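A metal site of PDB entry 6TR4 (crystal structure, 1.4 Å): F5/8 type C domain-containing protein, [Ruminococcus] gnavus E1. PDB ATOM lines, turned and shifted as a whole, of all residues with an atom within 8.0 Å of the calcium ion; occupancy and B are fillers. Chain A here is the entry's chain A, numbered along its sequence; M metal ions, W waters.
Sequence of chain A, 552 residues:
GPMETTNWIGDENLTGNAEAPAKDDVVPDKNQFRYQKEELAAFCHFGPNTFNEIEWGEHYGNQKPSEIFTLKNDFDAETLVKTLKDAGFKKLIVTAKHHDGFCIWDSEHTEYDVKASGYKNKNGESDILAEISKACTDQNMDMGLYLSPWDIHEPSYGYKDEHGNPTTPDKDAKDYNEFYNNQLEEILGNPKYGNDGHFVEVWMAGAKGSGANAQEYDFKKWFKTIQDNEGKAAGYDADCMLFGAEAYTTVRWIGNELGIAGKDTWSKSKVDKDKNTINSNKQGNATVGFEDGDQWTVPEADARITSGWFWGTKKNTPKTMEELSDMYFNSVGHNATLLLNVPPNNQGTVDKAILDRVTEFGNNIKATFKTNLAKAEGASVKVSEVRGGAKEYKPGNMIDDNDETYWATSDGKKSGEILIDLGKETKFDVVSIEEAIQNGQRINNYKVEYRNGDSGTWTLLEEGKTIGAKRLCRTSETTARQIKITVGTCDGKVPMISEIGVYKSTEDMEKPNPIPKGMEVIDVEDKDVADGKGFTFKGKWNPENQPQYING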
ATOM      1  N   GLU A 154     -29.517 -30.115 -19.429  1.00  0.00           N
ATOM      2  CA  GLU A 154     -29.149 -29.355 -20.653  1.00  0.00           C
ATOM      3  C   GLU A 154     -28.220 -28.203 -20.281  1.00  0.00           C
ATOM      4  O   GLU A 154     -28.591 -27.331 -19.490  1.00  0.00           O
ATOM      5  CB  GLU A 154     -30.422 -28.889 -21.343  1.00  0.00           C
ATOM      6  CG  GLU A 154     -30.209 -27.848 -22.411  1.00  0.00           C
ATOM      7  CD  GLU A 154     -29.142 -28.151 -23.452  1.00  0.00           C
ATOM      8  OE1 GLU A 154     -28.944 -29.343 -23.767  1.00  0.00           O
ATOM      9  OE2 GLU A 154     -28.527 -27.178 -23.972  1.00  0.00           O
ATOM     10  N   PRO A 155     -27.015 -28.121 -20.866  1.00  0.00           N
ATOM     11  CA  PRO A 155     -26.084 -27.041 -20.478  1.00  0.00           C
ATOM     12  C   PRO A 155     -26.604 -25.634 -20.753  1.00  0.00           C
ATOM     13  O   PRO A 155     -26.185 -24.733 -20.066  1.00  0.00           O
ATOM     14  CB  PRO A 155     -24.816 -27.296 -21.285  1.00  0.00           C
ATOM     15  CG  PRO A 155     -24.912 -28.753 -21.675  1.00  0.00           C
ATOM     16  CD  PRO A 155     -26.371 -29.123 -21.726  1.00  0.00           C
ATOM     17  N   SER A 156     -27.482 -25.440 -21.733  1.00  0.00           N
ATOM     18  CA  SER A 156     -28.023 -24.096 -22.038  1.00  0.00           C
ATOM     19  C   SER A 156     -28.966 -23.615 -20.939  1.00  0.00           C
ATOM     20  O   SER A 156     -29.277 -22.408 -20.928  1.00  0.00           O
ATOM     21  CB  SER A 156     -28.656 -24.002 -23.396  1.00  0.00           C
ATOM     22  OG  SER A 156     -29.810 -24.826 -23.514  1.00  0.00           O
ATOM     23  N   TYR A 157     -29.431 -24.482 -20.028  1.00  0.00           N
ATOM     24  CA  TYR A 157     -30.362 -24.056 -18.964  1.00  0.00           C
ATOM     25  C   TYR A 157     -29.617 -23.130 -17.993  1.00  0.00           C
ATOM     26  O   TYR A 157     -28.518 -23.457 -17.532  1.00  0.00           O
ATOM     27  CB  TYR A 157     -30.967 -25.244 -18.218  1.00  0.00           C
ATOM     28  CG  TYR A 157     -32.174 -24.840 -17.409  1.00  0.00           C
ATOM     29  CD1 TYR A 157     -33.439 -24.834 -17.976  1.00  0.00           C
ATOM     30  CD2 TYR A 157     -32.063 -24.393 -16.105  1.00  0.00           C
ATOM     31  CE1 TYR A 157     -34.552 -24.391 -17.275  1.00  0.00           C
ATOM     32  CE2 TYR A 157     -33.161 -23.960 -15.379  1.00  0.00           C
ATOM     33  CZ  TYR A 157     -34.423 -23.991 -15.951  1.00  0.00           C
ATOM     34  OH  TYR A 157     -35.517 -23.543 -15.259  1.00  0.00           O
ATOM     35  N   GLY A 158     -30.253 -22.001 -17.655  1.00  0.00           N
ATOM     36  CA  GLY A 158     -29.689 -21.016 -16.732  1.00  0.00           C
ATOM     37  C   GLY A 158     -28.707 -20.125 -17.432  1.00  0.00           C
ATOM     38  O   GLY A 158     -28.527 -20.208 -18.666  1.00  0.00           O
ATOM     39  N   TYR A 159     -28.090 -19.235 -16.670  1.00  0.00           N
ATOM     40  CA  TYR A 159     -27.203 -18.200 -17.245  1.00  0.00           C
ATOM     41  C   TYR A 159     -25.759 -18.594 -16.940  1.00  0.00           C
ATOM     42  O   TYR A 159     -25.354 -18.541 -15.782  1.00  0.00           O
ATOM     43  CB  TYR A 159     -27.591 -16.821 -16.719  1.00  0.00           C
ATOM     44  CG  TYR A 159     -29.061 -16.503 -16.838  1.00  0.00           C
ATOM     45  CD1 TYR A 159     -29.726 -16.565 -18.048  1.00  0.00           C
ATOM     46  CD2 TYR A 159     -29.796 -16.179 -15.719  1.00  0.00           C
ATOM     47  CE1 TYR A 159     -31.074 -16.281 -18.158  1.00  0.00           C
ATOM     48  CE2 TYR A 159     -31.140 -15.857 -15.803  1.00  0.00           C
ATOM     49  CZ  TYR A 159     -31.793 -15.949 -17.025  1.00  0.00           C
ATOM     50  OH  TYR A 159     -33.129 -15.680 -17.119  1.00  0.00           O
ATOM     51  N   LYS A 160     -25.047 -19.044 -17.979  1.00  0.00           N
ATOM     52  CA  LYS A 160     -23.672 -19.580 -17.822  1.00  0.00           C
ATOM     53  C   LYS A 160     -22.799 -19.031 -18.941  1.00  0.00           C
ATOM     54  O   LYS A 160     -23.265 -18.884 -20.078  1.00  0.00           O
ATOM     55  CB  LYS A 160     -23.693 -21.118 -17.808  1.00  0.00           C
ATOM     56  CG  LYS A 160     -24.478 -21.743 -16.657  1.00  0.00           C
ATOM     57  CD  LYS A 160     -24.525 -23.270 -16.784  1.00  0.00           C
ATOM     58  CE  LYS A 160     -25.695 -23.948 -16.108  1.00  0.00           C
ATOM     59  NZ  LYS A 160     -26.304 -25.036 -16.931  1.00  0.00           N
ATOM     60  N   ASP A 161     -21.560 -18.723 -18.613  1.00  0.00           N
ATOM     61  CA  ASP A 161     -20.621 -18.159 -19.621  1.00  0.00           C
ATOM     62  C   ASP A 161     -20.042 -19.291 -20.468  1.00  0.00           C
ATOM     63  O   ASP A 161     -20.456 -20.445 -20.312  1.00  0.00           O
ATOM     64  CB  ASP A 161     -19.546 -17.329 -18.917  1.00  0.00           C
ATOM     65  CG  ASP A 161     -18.588 -18.089 -18.013  1.00  0.00           C
ATOM     66  OD1 ASP A 161     -18.585 -19.347 -18.033  1.00  0.00           O
ATOM     67  OD2 ASP A 161     -17.821 -17.392 -17.297  1.00  0.00           O
ATOM     68  N   THR A 167     -23.222 -16.717 -14.630  1.00  0.00           N
ATOM     69  CA  THR A 167     -23.050 -15.323 -15.106  1.00  0.00           C
ATOM     70  C   THR A 167     -24.423 -14.665 -15.150  1.00  0.00           C
ATOM     71  O   THR A 167     -25.427 -15.282 -14.718  1.00  0.00           O
ATOM     72  CB  THR A 167     -22.280 -15.274 -16.436  1.00  0.00           C
ATOM     73  OG1 THR A 167     -21.891 -13.914 -16.638  1.00  0.00           O
ATOM     74  CG2 THR A 167     -23.075 -15.801 -17.600  1.00  0.00           C
ATOM     75  N   THR A 168     -24.446 -13.482 -15.722  1.00  0.00           N
ATOM     76  CA  THR A 168     -25.678 -12.689 -15.885  1.00  0.00           C
ATOM     77  C   THR A 168     -26.245 -12.965 -17.279  1.00  0.00           C
ATOM     78  O   THR A 168     -25.559 -13.464 -18.184  1.00  0.00           O
ATOM     79  CB  THR A 168     -25.371 -11.211 -15.625  1.00  0.00           C
ATOM     80  OG1 THR A 168     -24.103 -10.905 -16.179  1.00  0.00           O
ATOM     81  CG2 THR A 168     -25.341 -10.882 -14.150  1.00  0.00           C
ATOM     82  N   PRO A 169     -27.544 -12.661 -17.492  1.00  0.00           N
ATOM     83  CA  PRO A 169     -28.190 -13.018 -18.772  1.00  0.00           C
ATOM     84  C   PRO A 169     -27.481 -12.511 -20.034  1.00  0.00           C
ATOM     85  O   PRO A 169     -27.479 -13.200 -21.028  1.00  0.00           O
ATOM     86  CB  PRO A 169     -29.574 -12.405 -18.594  1.00  0.00           C
ATOM     87  CG  PRO A 169     -29.826 -12.542 -17.124  1.00  0.00           C
ATOM     88  CD  PRO A 169     -28.501 -12.184 -16.482  1.00  0.00           C
ATOM     89  N   LYS A 171     -24.364 -12.279 -20.645  1.00  0.00           N
ATOM     90  CA  LYS A 171     -23.103 -13.028 -20.905  1.00  0.00           C
ATOM     91  C   LYS A 171     -23.390 -14.518 -21.045  1.00  0.00           C
ATOM     92  O   LYS A 171     -22.433 -15.305 -21.191  1.00  0.00           O
ATOM     93  CB  LYS A 171     -22.099 -12.718 -19.785  1.00  0.00           C
ATOM     94  CG  LYS A 171     -21.625 -11.274 -19.776  1.00  0.00           C
ATOM     95  CD  LYS A 171     -20.729 -10.878 -18.613  1.00  0.00           C
ATOM     96  CE  LYS A 171     -20.150  -9.483 -18.762  1.00  0.00           C
ATOM     97  NZ  LYS A 171     -21.158  -8.427 -18.494  1.00  0.00           N
ATOM     98  N   ASP A 172     -24.663 -14.893 -21.032  1.00  0.00           N
ATOM     99  CA  ASP A 172     -25.077 -16.300 -21.194  1.00  0.00           C
ATOM    100  C   ASP A 172     -24.678 -16.744 -22.601  1.00  0.00           C
ATOM    101  O   ASP A 172     -25.126 -16.129 -23.585  1.00  0.00           O
ATOM    102  CB  ASP A 172     -26.576 -16.397 -20.972  1.00  0.00           C
ATOM    103  CG  ASP A 172     -27.118 -17.805 -21.023  1.00  0.00           C
ATOM    104  OD1 ASP A 172     -26.422 -18.740 -20.560  1.00  0.00           O
ATOM    105  OD2 ASP A 172     -28.243 -17.953 -21.509  1.00  0.00           O
ATOM    106  N   ALA A 173     -23.877 -17.792 -22.708  1.00  0.00           N
ATOM    107  CA  ALA A 173     -23.329 -18.225 -24.008  1.00  0.00           C
ATOM    108  C   ALA A 173     -24.360 -18.977 -24.834  1.00  0.00           C
ATOM    109  O   ALA A 173     -24.300 -18.852 -26.077  1.00  0.00           O
ATOM    110  CB  ALA A 173     -22.113 -19.074 -23.784  1.00  0.00           C
ATOM    111  N   LYS A 174     -25.215 -19.780 -24.196  1.00  0.00           N
ATOM    112  CA  LYS A 174     -26.187 -20.656 -24.914  1.00  0.00           C
ATOM    113  C   LYS A 174     -27.589 -20.436 -24.337  1.00  0.00           C
ATOM    114  O   LYS A 174     -27.772 -20.577 -23.109  1.00  0.00           O
ATOM    115  CB  LYS A 174     -25.764 -22.118 -24.800  1.00  0.00           C
ATOM    116  CG  LYS A 174     -24.397 -22.446 -25.387  1.00  0.00           C
ATOM    117  CD  LYS A 174     -24.378 -22.531 -26.896  1.00  0.00           C
ATOM    118  CE  LYS A 174     -23.017 -22.959 -27.436  1.00  0.00           C
ATOM    119  NZ  LYS A 174     -22.996 -23.083 -28.912  1.00  0.00           N
ATOM    120  N   ASP A 175     -28.525 -20.097 -25.207  1.00  0.00           N
ATOM    121  CA  ASP A 175     -29.894 -19.669 -24.809  1.00  0.00           C
ATOM    122  C   ASP A 175     -30.805 -20.885 -24.729  1.00  0.00           C
ATOM    123  O   ASP A 175     -31.126 -21.493 -25.764  1.00  0.00           O
ATOM    124  CB  ASP A 175     -30.461 -18.666 -25.808  1.00  0.00           C
ATOM    125  CG  ASP A 175     -31.733 -18.004 -25.337  1.00  0.00           C
ATOM    126  OD1 ASP A 175     -32.321 -18.460 -24.320  1.00  0.00           O
ATOM    127  OD2 ASP A 175     -32.104 -16.956 -25.965  1.00  0.00           O
ATOM    128  N   TYR A 176     -31.256 -21.227 -23.527  1.00  0.00           N
ATOM    129  CA  TYR A 176     -32.183 -22.362 -23.329  1.00  0.00           C
ATOM    130  C   TYR A 176     -33.474 -22.140 -24.104  1.00  0.00           C
ATOM    131  O   TYR A 176     -34.094 -23.123 -24.546  1.00  0.00           O
ATOM    132  CB  TYR A 176     -32.521 -22.507 -21.857  1.00  0.00           C
ATOM    133  CG  TYR A 176     -33.442 -23.669 -21.585  1.00  0.00           C
ATOM    134  CD1 TYR A 176     -32.983 -24.955 -21.766  1.00  0.00           C
ATOM    135  CD2 TYR A 176     -34.760 -23.471 -21.223  1.00  0.00           C
ATOM    136  CE1 TYR A 176     -33.819 -26.036 -21.549  1.00  0.00           C
ATOM    137  CE2 TYR A 176     -35.606 -24.542 -21.008  1.00  0.00           C
ATOM    138  CZ  TYR A 176     -35.128 -25.825 -21.161  1.00  0.00           C
ATOM    139  OH  TYR A 176     -35.949 -26.907 -20.925  1.00  0.00           O
ATOM    140  N   ASN A 177     -33.937 -20.901 -24.247  1.00  0.00           N
ATOM    141  CA  ASN A 177     -35.205 -20.629 -24.974  1.00  0.00           C
ATOM    142  C   ASN A 177     -35.075 -21.106 -26.415  1.00  0.00           C
ATOM    143  O   ASN A 177     -36.084 -21.557 -26.958  1.00  0.00           O
ATOM    144  CB  ASN A 177     -35.596 -19.172 -24.893  1.00  0.00           C
ATOM    145  CG  ASN A 177     -36.126 -18.876 -23.510  1.00  0.00           C
ATOM    146  OD1 ASN A 177     -36.966 -19.620 -23.008  1.00  0.00           O
ATOM    147  ND2 ASN A 177     -35.652 -17.834 -22.875  1.00  0.00           N
ATOM    148  N   ALA A 214     -32.009 -19.848 -12.060  1.00  0.00           N
ATOM    149  CA  ALA A 214     -32.975 -18.928 -12.687  1.00  0.00           C
ATOM    150  C   ALA A 214     -32.947 -19.111 -14.206  1.00  0.00           C
ATOM    151  O   ALA A 214     -31.842 -19.326 -14.792  1.00  0.00           O
ATOM    152  CB  ALA A 214     -32.674 -17.501 -12.336  1.00  0.00           C
ATOM    153  N   GLN A 215     -34.121 -19.065 -14.819  1.00  0.00           N
ATOM    154  CA  GLN A 215     -34.238 -19.129 -16.299  1.00  0.00           C
ATOM    155  C   GLN A 215     -35.587 -18.549 -16.697  1.00  0.00           C
ATOM    156  O   GLN A 215     -36.611 -19.160 -16.417  1.00  0.00           O
ATOM    157  CB  GLN A 215     -34.096 -20.563 -16.795  1.00  0.00           C
ATOM    158  CG  GLN A 215     -34.310 -20.716 -18.297  1.00  0.00           C
ATOM    159  CD  GLN A 215     -33.243 -20.028 -19.122  1.00  0.00           C
ATOM    160  OE1 GLN A 215     -32.081 -20.428 -19.104  1.00  0.00           O
ATOM    161  NE2 GLN A 215     -33.635 -18.985 -19.860  1.00  0.00           N
HETATM  162 CA    CA M   1     -28.094 -20.398 -20.894  1.00  0.00          CA
HETATM  163  O   HOH W   1     -30.483 -19.706 -21.121  1.00  0.00           O
HETATM  164  O   HOH W   2     -26.406 -21.848 -20.223  1.00  0.00           O
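The backbone NH (N) of Gly 158 sits at hydrogen-bond distance from the side-chain amide oxygen (OE1) of Gln 215, 2.8 Å away. The backbone NH of Tyr 176 sits close to the backbone carbonyl oxygen of Ser 156 (3.5 Å). The side-chain carboxylate (OE2) of Glu 154 lies within hydrogen-bond range of the side-chain hydroxyl (OG) of Ser 156. The side-chain carboxylate (OD1) of Asp 172 lies close to the backbone NH (N) of Lys 160.
The calcium ion is bound by O of Lys 174 (2.2 Å), O of Gly 158 (2.3 Å), water W2 (2.3 Å), O of Ser 156 (2.3 Å), OD1 of Asp 172 (2.4 Å), water W1 (2.5 Å) and OD2 of Asp 172 (2.5 Å).
Water W1 lies within hydrogen-bond range of OE1 of Gln 215 (2.7 Å) and N of Tyr 176 (2.9 Å).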
